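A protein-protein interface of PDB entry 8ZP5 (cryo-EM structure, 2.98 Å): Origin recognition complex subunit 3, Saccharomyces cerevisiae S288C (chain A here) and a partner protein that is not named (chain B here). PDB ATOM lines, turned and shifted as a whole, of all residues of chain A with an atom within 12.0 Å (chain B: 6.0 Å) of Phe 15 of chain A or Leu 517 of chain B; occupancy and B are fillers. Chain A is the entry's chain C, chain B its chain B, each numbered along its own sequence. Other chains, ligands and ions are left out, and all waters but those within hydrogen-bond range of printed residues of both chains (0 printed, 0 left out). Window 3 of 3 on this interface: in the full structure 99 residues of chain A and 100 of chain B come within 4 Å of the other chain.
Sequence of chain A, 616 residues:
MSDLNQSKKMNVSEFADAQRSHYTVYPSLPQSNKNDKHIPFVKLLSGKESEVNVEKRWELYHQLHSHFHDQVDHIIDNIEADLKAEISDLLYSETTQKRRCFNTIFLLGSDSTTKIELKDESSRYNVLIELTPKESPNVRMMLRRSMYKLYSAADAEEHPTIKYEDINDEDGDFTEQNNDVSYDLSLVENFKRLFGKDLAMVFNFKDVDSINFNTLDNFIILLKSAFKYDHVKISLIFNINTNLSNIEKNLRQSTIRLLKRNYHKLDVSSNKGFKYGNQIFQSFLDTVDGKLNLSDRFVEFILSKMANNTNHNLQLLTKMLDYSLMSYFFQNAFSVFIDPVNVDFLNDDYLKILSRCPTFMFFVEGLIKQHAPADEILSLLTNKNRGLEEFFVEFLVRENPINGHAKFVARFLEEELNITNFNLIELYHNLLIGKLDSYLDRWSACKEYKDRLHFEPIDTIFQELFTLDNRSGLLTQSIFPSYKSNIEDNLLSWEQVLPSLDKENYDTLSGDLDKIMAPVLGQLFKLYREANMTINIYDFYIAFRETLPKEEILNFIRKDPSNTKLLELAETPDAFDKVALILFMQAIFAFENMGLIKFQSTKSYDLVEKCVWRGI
Phe 15 of chain A touches four residues of chain B. Leu 517 of chain B touches just one residue of chain A: Phe 15. No residue of chain A comes within 4 Å of Val 513 of chain B. No residue of chain A comes within 4 Å of Leu 514 of chain B. Of chain A, only Phe 15 comes within 4 Å of Ser 516 of chain B. No residue of chain A comes within 4 Å of Thr 518 of chain B. No residue of chain A comes within 4 Å of Lys 522 of chain B. Printed residues of chain B within 4 Å of Gln 19 of chain A: His 585 (3.8 Å). Printed residues of chain A within 4 Å of His 585 of chain B: Phe 15, Ala 16 and Gln 19. The nearest residue of chain B that does not touch Phe 15 of chain A is Thr 518 of chain B (4.1 Å). The nearest residue of chain A that does not touch Leu 517 of chain B is Ala 16 of chain A (7.9 Å).
The side-chain carboxylate (OE2) of Glu 581 of chain B lies close to the backbone NH (N) of Phe 15 of chain A.
Printed residues of chain A that touch a printed residue of chain B: Phe 15, Ala 16 and Gln 19.
Ser 516 of chain B touches Phe 15 of chain A. CE2 of Phe 15 of chain A touches CA of Leu 517 of chain B (3.9 Å). Phe 15 of chain A touches His 585 of chain B. O of Ala 16 of chain A touches CE1 of His 585 of chain B, at 3.8 Å. Gln 19 of chain A touches His 585 of chain B (O to ND1, 3.8 Å).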
ATOM      1  N   PHE A  15      -8.496 -11.560  21.795  1.00  0.00           N
ATOM      2  CA  PHE A  15      -7.417 -10.667  22.199  1.00  0.00           C
ATOM      3  C   PHE A  15      -6.319 -11.418  22.943  1.00  0.00           C
ATOM      4  O   PHE A  15      -5.172 -11.461  22.500  1.00  0.00           O
ATOM      5  CB  PHE A  15      -7.955  -9.532  23.074  1.00  0.00           C
ATOM      6  CG  PHE A  15      -8.713  -8.483  22.312  1.00  0.00           C
ATOM      7  CD1 PHE A  15      -8.618  -8.403  20.933  1.00  0.00           C
ATOM      8  CD2 PHE A  15      -9.515  -7.571  22.977  1.00  0.00           C
ATOM      9  CE1 PHE A  15      -9.313  -7.436  20.231  1.00  0.00           C
ATOM     10  CE2 PHE A  15     -10.212  -6.602  22.282  1.00  0.00           C
ATOM     11  CZ  PHE A  15     -10.110  -6.535  20.907  1.00  0.00           C
ATOM     12  N   ALA A  16      -6.680 -12.006  24.081  1.00  0.00           N
ATOM     13  CA  ALA A  16      -5.707 -12.706  24.907  1.00  0.00           C
ATOM     14  C   ALA A  16      -5.195 -13.952  24.198  1.00  0.00           C
ATOM     15  O   ALA A  16      -5.949 -14.664  23.531  1.00  0.00           O
ATOM     16  CB  ALA A  16      -6.325 -13.081  26.252  1.00  0.00           C
ATOM     17  N   ASP A  17      -3.893 -14.212  24.349  1.00  0.00           N
ATOM     18  CA  ASP A  17      -3.301 -15.399  23.744  1.00  0.00           C
ATOM     19  C   ASP A  17      -3.687 -16.664  24.497  1.00  0.00           C
ATOM     20  O   ASP A  17      -3.725 -17.749  23.904  1.00  0.00           O
ATOM     21  CB  ASP A  17      -1.780 -15.257  23.690  1.00  0.00           C
ATOM     22  CG  ASP A  17      -1.306 -14.540  22.441  1.00  0.00           C
ATOM     23  OD1 ASP A  17      -2.086 -14.454  21.470  1.00  0.00           O
ATOM     24  OD2 ASP A  17      -0.152 -14.064  22.431  1.00  0.00           O
ATOM     25  N   ALA A  18      -3.971 -16.548  25.796  1.00  0.00           N
ATOM     26  CA  ALA A  18      -4.363 -17.715  26.578  1.00  0.00           C
ATOM     27  C   ALA A  18      -5.706 -18.273  26.126  1.00  0.00           C
ATOM     28  O   ALA A  18      -5.925 -19.487  26.195  1.00  0.00           O
ATOM     29  CB  ALA A  18      -4.413 -17.359  28.062  1.00  0.00           C
ATOM     30  N   GLN A  19      -6.611 -17.412  25.667  1.00  0.00           N
ATOM     31  CA  GLN A  19      -7.920 -17.848  25.199  1.00  0.00           C
ATOM     32  C   GLN A  19      -7.879 -18.440  23.798  1.00  0.00           C
ATOM     33  O   GLN A  19      -8.890 -18.984  23.344  1.00  0.00           O
ATOM     34  CB  GLN A  19      -8.908 -16.680  25.234  1.00  0.00           C
ATOM     35  CG  GLN A  19      -8.821 -15.835  26.492  1.00  0.00           C
ATOM     36  CD  GLN A  19      -9.034 -16.646  27.752  1.00  0.00           C
ATOM     37  OE1 GLN A  19      -9.863 -17.555  27.786  1.00  0.00           O
ATOM     38  NE2 GLN A  19      -8.283 -16.322  28.798  1.00  0.00           N
ATOM     39  N   ARG A  20      -6.746 -18.347  23.111  1.00  0.00           N
ATOM     40  CA  ARG A  20      -6.583 -18.897  21.776  1.00  0.00           C
ATOM     41  C   ARG A  20      -6.013 -20.308  21.862  1.00  0.00           C
ATOM     42  O   ARG A  20      -5.401 -20.689  22.862  1.00  0.00           O
ATOM     43  CB  ARG A  20      -5.662 -18.012  20.933  1.00  0.00           C
ATOM     44  CG  ARG A  20      -5.801 -18.212  19.435  1.00  0.00           C
ATOM     45  CD  ARG A  20      -4.574 -17.714  18.697  1.00  0.00           C
ATOM     46  NE  ARG A  20      -4.092 -16.449  19.238  1.00  0.00           N
ATOM     47  CZ  ARG A  20      -4.387 -15.259  18.734  1.00  0.00           C
ATOM     48  NH1 ARG A  20      -5.166 -15.132  17.673  1.00  0.00           N
ATOM     49  NH2 ARG A  20      -3.887 -14.169  19.310  1.00  0.00           N
ATOM     50  N   SER A  21      -6.228 -21.081  20.803  1.00  0.00           N
ATOM     51  CA  SER A  21      -5.685 -22.428  20.693  1.00  0.00           C
ATOM     52  C   SER A  21      -4.502 -22.419  19.735  1.00  0.00           C
ATOM     53  O   SER A  21      -4.558 -21.774  18.683  1.00  0.00           O
ATOM     54  CB  SER A  21      -6.752 -23.409  20.210  1.00  0.00           C
ATOM     55  OG  SER A  21      -7.479 -22.870  19.120  1.00  0.00           O
ATOM     56  N   HIS A  22      -3.434 -23.118  20.115  1.00  0.00           N
ATOM     57  CA  HIS A  22      -2.240 -23.324  19.292  1.00  0.00           C
ATOM     58  C   HIS A  22      -1.715 -22.005  18.709  1.00  0.00           C
ATOM     59  O   HIS A  22      -1.643 -21.796  17.499  1.00  0.00           O
ATOM     60  CB  HIS A  22      -2.508 -24.376  18.205  1.00  0.00           C
ATOM     61  CG  HIS A  22      -3.378 -23.903  17.081  1.00  0.00           C
ATOM     62  ND1 HIS A  22      -2.908 -23.098  16.066  1.00  0.00           N
ATOM     63  CD2 HIS A  22      -4.684 -24.130  16.807  1.00  0.00           C
ATOM     64  CE1 HIS A  22      -3.889 -22.843  15.218  1.00  0.00           C
ATOM     65  NE2 HIS A  22      -4.978 -23.458  15.646  1.00  0.00           N
ATOM     66  N   TYR A  23      -1.322 -21.118  19.616  1.00  0.00           N
ATOM     67  CA  TYR A  23      -0.686 -19.864  19.235  1.00  0.00           C
ATOM     68  C   TYR A  23       0.827 -20.033  19.305  1.00  0.00           C
ATOM     69  O   TYR A  23       1.365 -20.451  20.335  1.00  0.00           O
ATOM     70  CB  TYR A  23      -1.149 -18.711  20.129  1.00  0.00           C
ATOM     71  CG  TYR A  23      -0.646 -18.758  21.554  1.00  0.00           C
ATOM     72  CD1 TYR A  23      -1.226 -19.601  22.489  1.00  0.00           C
ATOM     73  CD2 TYR A  23       0.403 -17.949  21.964  1.00  0.00           C
ATOM     74  CE1 TYR A  23      -0.770 -19.641  23.790  1.00  0.00           C
ATOM     75  CE2 TYR A  23       0.865 -17.982  23.261  1.00  0.00           C
ATOM     76  CZ  TYR A  23       0.276 -18.829  24.171  1.00  0.00           C
ATOM     77  OH  TYR A  23       0.735 -18.865  25.466  1.00  0.00           O
ATOM     78  N   THR A  24       1.504 -19.730  18.203  1.00  0.00           N
ATOM     79  CA  THR A  24       2.946 -19.915  18.121  1.00  0.00           C
ATOM     80  C   THR A  24       3.681 -18.709  18.689  1.00  0.00           C
ATOM     81  O   THR A  24       3.267 -17.562  18.496  1.00  0.00           O
ATOM     82  CB  THR A  24       3.374 -20.148  16.672  1.00  0.00           C
ATOM     83  OG1 THR A  24       2.576 -21.191  16.101  1.00  0.00           O
ATOM     84  CG2 THR A  24       4.833 -20.552  16.610  1.00  0.00           C
ATOM     85  N   VAL A  25       4.781 -18.974  19.389  1.00  0.00           N
ATOM     86  CA  VAL A  25       5.601 -17.941  20.006  1.00  0.00           C
ATOM     87  C   VAL A  25       7.015 -18.054  19.457  1.00  0.00           C
ATOM     88  O   VAL A  25       7.563 -19.159  19.365  1.00  0.00           O
ATOM     89  CB  VAL A  25       5.606 -18.060  21.541  1.00  0.00           C
ATOM     90  CG1 VAL A  25       6.437 -16.948  22.159  1.00  0.00           C
ATOM     91  CG2 VAL A  25       4.189 -18.033  22.079  1.00  0.00           C
ATOM     92  N   ALA B 510     -16.212 -18.356  24.720  1.00  0.00           N
ATOM     93  CA  ALA B 510     -16.726 -17.333  23.817  1.00  0.00           C
ATOM     94  C   ALA B 510     -17.271 -16.142  24.592  1.00  0.00           C
ATOM     95  O   ALA B 510     -16.966 -14.990  24.270  1.00  0.00           O
ATOM     96  CB  ALA B 510     -17.806 -17.926  22.914  1.00  0.00           C
ATOM     97  N   VAL B 513     -14.505 -14.099  26.035  1.00  0.00           N
ATOM     98  CA  VAL B 513     -13.999 -13.217  24.986  1.00  0.00           C
ATOM     99  C   VAL B 513     -14.934 -12.029  24.792  1.00  0.00           C
ATOM    100  O   VAL B 513     -14.486 -10.895  24.579  1.00  0.00           O
ATOM    101  CB  VAL B 513     -13.792 -14.003  23.676  1.00  0.00           C
ATOM    102  CG1 VAL B 513     -13.332 -13.076  22.571  1.00  0.00           C
ATOM    103  CG2 VAL B 513     -12.768 -15.105  23.877  1.00  0.00           C
ATOM    104  N   LEU B 514     -16.247 -12.267  24.877  1.00  0.00           N
ATOM    105  CA  LEU B 514     -17.217 -11.215  24.569  1.00  0.00           C
ATOM    106  C   LEU B 514     -17.217 -10.066  25.568  1.00  0.00           C
ATOM    107  O   LEU B 514     -17.593  -8.950  25.192  1.00  0.00           O
ATOM    108  CB  LEU B 514     -18.634 -11.779  24.449  1.00  0.00           C
ATOM    109  CG  LEU B 514     -19.134 -12.116  23.041  1.00  0.00           C
ATOM    110  CD1 LEU B 514     -19.250 -10.841  22.231  1.00  0.00           C
ATOM    111  CD2 LEU B 514     -18.225 -13.064  22.325  1.00  0.00           C
ATOM    112  N   GLN B 515     -16.839 -10.281  26.834  1.00  0.00           N
ATOM    113  CA  GLN B 515     -16.715  -9.090  27.688  1.00  0.00           C
ATOM    114  C   GLN B 515     -15.631  -8.144  27.184  1.00  0.00           C
ATOM    115  O   GLN B 515     -15.792  -6.920  27.259  1.00  0.00           O
ATOM    116  CB  GLN B 515     -16.462  -9.406  29.165  1.00  0.00           C
ATOM    117  CG  GLN B 515     -17.595 -10.078  29.903  1.00  0.00           C
ATOM    118  CD  GLN B 515     -17.627 -11.551  29.693  1.00  0.00           C
ATOM    119  OE1 GLN B 515     -16.642 -12.130  29.267  1.00  0.00           O
ATOM    120  NE2 GLN B 515     -18.754 -12.174  30.000  1.00  0.00           N
ATOM    121  N   SER B 516     -14.517  -8.677  26.692  1.00  0.00           N
ATOM    122  CA  SER B 516     -13.396  -7.849  26.243  1.00  0.00           C
ATOM    123  C   SER B 516     -13.336  -7.870  24.714  1.00  0.00           C
ATOM    124  O   SER B 516     -12.583  -8.641  24.117  1.00  0.00           O
ATOM    125  CB  SER B 516     -12.085  -8.331  26.855  1.00  0.00           C
ATOM    126  OG  SER B 516     -11.615  -9.500  26.211  1.00  0.00           O
ATOM    127  N   LEU B 517     -14.128  -7.003  24.087  1.00  0.00           N
ATOM    128  CA  LEU B 517     -14.131  -6.845  22.638  1.00  0.00           C
ATOM    129  C   LEU B 517     -14.561  -5.425  22.303  1.00  0.00           C
ATOM    130  O   LEU B 517     -15.153  -4.725  23.128  1.00  0.00           O
ATOM    131  CB  LEU B 517     -15.063  -7.852  21.952  1.00  0.00           C
ATOM    132  CG  LEU B 517     -14.571  -9.285  21.748  1.00  0.00           C
ATOM    133  CD1 LEU B 517     -15.681 -10.157  21.188  1.00  0.00           C
ATOM    134  CD2 LEU B 517     -13.362  -9.303  20.829  1.00  0.00           C
ATOM    135  N   THR B 518     -14.255  -5.013  21.077  1.00  0.00           N
ATOM    136  CA  THR B 518     -14.719  -3.728  20.577  1.00  0.00           C
ATOM    137  C   THR B 518     -16.237  -3.742  20.422  1.00  0.00           C
ATOM    138  O   THR B 518     -16.848  -4.787  20.188  1.00  0.00           O
ATOM    139  CB  THR B 518     -14.052  -3.413  19.238  1.00  0.00           C
ATOM    140  OG1 THR B 518     -12.658  -3.729  19.320  1.00  0.00           O
ATOM    141  CG2 THR B 518     -14.201  -1.942  18.898  1.00  0.00           C
ATOM    142  N   VAL B 519     -16.846  -2.563  20.567  1.00  0.00           N
ATOM    143  CA  VAL B 519     -18.300  -2.470  20.493  1.00  0.00           C
ATOM    144  C   VAL B 519     -18.797  -2.832  19.097  1.00  0.00           C
ATOM    145  O   VAL B 519     -19.857  -3.449  18.944  1.00  0.00           O
ATOM    146  CB  VAL B 519     -18.769  -1.069  20.928  1.00  0.00           C
ATOM    147  CG1 VAL B 519     -18.198   0.011  20.017  1.00  0.00           C
ATOM    148  CG2 VAL B 519     -20.287  -1.004  20.960  1.00  0.00           C
ATOM    149  N   SER B 521     -17.337  -4.998  17.021  1.00  0.00           N
ATOM    150  CA  SER B 521     -17.255  -6.451  16.927  1.00  0.00           C
ATOM    151  C   SER B 521     -18.383  -7.115  17.705  1.00  0.00           C
ATOM    152  O   SER B 521     -18.954  -8.114  17.255  1.00  0.00           O
ATOM    153  CB  SER B 521     -15.896  -6.935  17.431  1.00  0.00           C
ATOM    154  OG  SER B 521     -14.850  -6.475  16.596  1.00  0.00           O
ATOM    155  N   LYS B 522     -18.717  -6.571  18.878  1.00  0.00           N
ATOM    156  CA  LYS B 522     -19.825  -7.115  19.656  1.00  0.00           C
ATOM    157  C   LYS B 522     -21.144  -6.980  18.906  1.00  0.00           C
ATOM    158  O   LYS B 522     -21.954  -7.911  18.892  1.00  0.00           O
ATOM    159  CB  LYS B 522     -19.907  -6.420  21.014  1.00  0.00           C
ATOM    160  CG  LYS B 522     -19.093  -7.094  22.105  1.00  0.00           C
ATOM    161  CD  LYS B 522     -19.269  -6.390  23.439  1.00  0.00           C
ATOM    162  CE  LYS B 522     -18.461  -5.105  23.493  1.00  0.00           C
ATOM    163  NZ  LYS B 522     -18.248  -4.639  24.891  1.00  0.00           N
ATOM    164  N   GLU B 581     -10.728 -12.419  13.621  1.00  0.00           N
ATOM    165  CA  GLU B 581     -10.531 -12.676  15.045  1.00  0.00           C
ATOM    166  C   GLU B 581     -11.467 -13.767  15.547  1.00  0.00           C
ATOM    167  O   GLU B 581     -11.056 -14.646  16.311  1.00  0.00           O
ATOM    168  CB  GLU B 581     -10.730 -11.391  15.845  1.00  0.00           C
ATOM    169  CG  GLU B 581     -10.550 -11.572  17.343  1.00  0.00           C
ATOM    170  CD  GLU B 581     -10.814 -10.303  18.124  1.00  0.00           C
ATOM    171  OE1 GLU B 581     -11.171  -9.280  17.502  1.00  0.00           O
ATOM    172  OE2 GLU B 581     -10.661 -10.327  19.364  1.00  0.00           O
ATOM    173  N   PHE B 582     -12.735 -13.727  15.129  1.00  0.00           N
ATOM    174  CA  PHE B 582     -13.690 -14.734  15.575  1.00  0.00           C
ATOM    175  C   PHE B 582     -13.387 -16.099  14.970  1.00  0.00           C
ATOM    176  O   PHE B 582     -13.587 -17.129  15.622  1.00  0.00           O
ATOM    177  CB  PHE B 582     -15.113 -14.291  15.237  1.00  0.00           C
ATOM    178  CG  PHE B 582     -15.587 -13.122  16.050  1.00  0.00           C
ATOM    179  CD1 PHE B 582     -15.871 -13.270  17.395  1.00  0.00           C
ATOM    180  CD2 PHE B 582     -15.735 -11.874  15.475  1.00  0.00           C
ATOM    181  CE1 PHE B 582     -16.304 -12.199  18.149  1.00  0.00           C
ATOM    182  CE2 PHE B 582     -16.165 -10.798  16.226  1.00  0.00           C
ATOM    183  CZ  PHE B 582     -16.451 -10.961  17.564  1.00  0.00           C
ATOM    184  N   HIS B 585     -10.265 -17.615  16.837  1.00  0.00           N
ATOM    185  CA  HIS B 585     -10.644 -18.090  18.161  1.00  0.00           C
ATOM    186  C   HIS B 585     -11.656 -19.229  18.113  1.00  0.00           C
ATOM    187  O   HIS B 585     -12.195 -19.600  19.162  1.00  0.00           O
ATOM    188  CB  HIS B 585     -11.206 -16.933  18.990  1.00  0.00           C
ATOM    189  CG  HIS B 585     -10.156 -16.100  19.656  1.00  0.00           C
ATOM    190  ND1 HIS B 585      -9.902 -16.165  21.008  1.00  0.00           N
ATOM    191  CD2 HIS B 585      -9.296 -15.183  19.154  1.00  0.00           C
ATOM    192  CE1 HIS B 585      -8.931 -15.322  21.312  1.00  0.00           C
ATOM    193  NE2 HIS B 585      -8.545 -14.715  20.204  1.00  0.00           N
ATOM    194  N   MET B 587     -14.663 -19.237  17.028  1.00  0.00           N
ATOM    195  CA  MET B 587     -15.966 -18.729  17.434  1.00  0.00           C
ATOM    196  C   MET B 587     -16.982 -18.734  16.303  1.00  0.00           C
ATOM    197  O   MET B 587     -18.152 -19.058  16.527  1.00  0.00           O
ATOM    198  CB  MET B 587     -15.822 -17.308  17.977  1.00  0.00           C
ATOM    199  CG  MET B 587     -15.043 -17.222  19.271  1.00  0.00           C
ATOM    200  SD  MET B 587     -15.164 -15.570  19.952  1.00  0.00           S
ATOM    201  CE  MET B 587     -16.890 -15.577  20.392  1.00  0.00           C
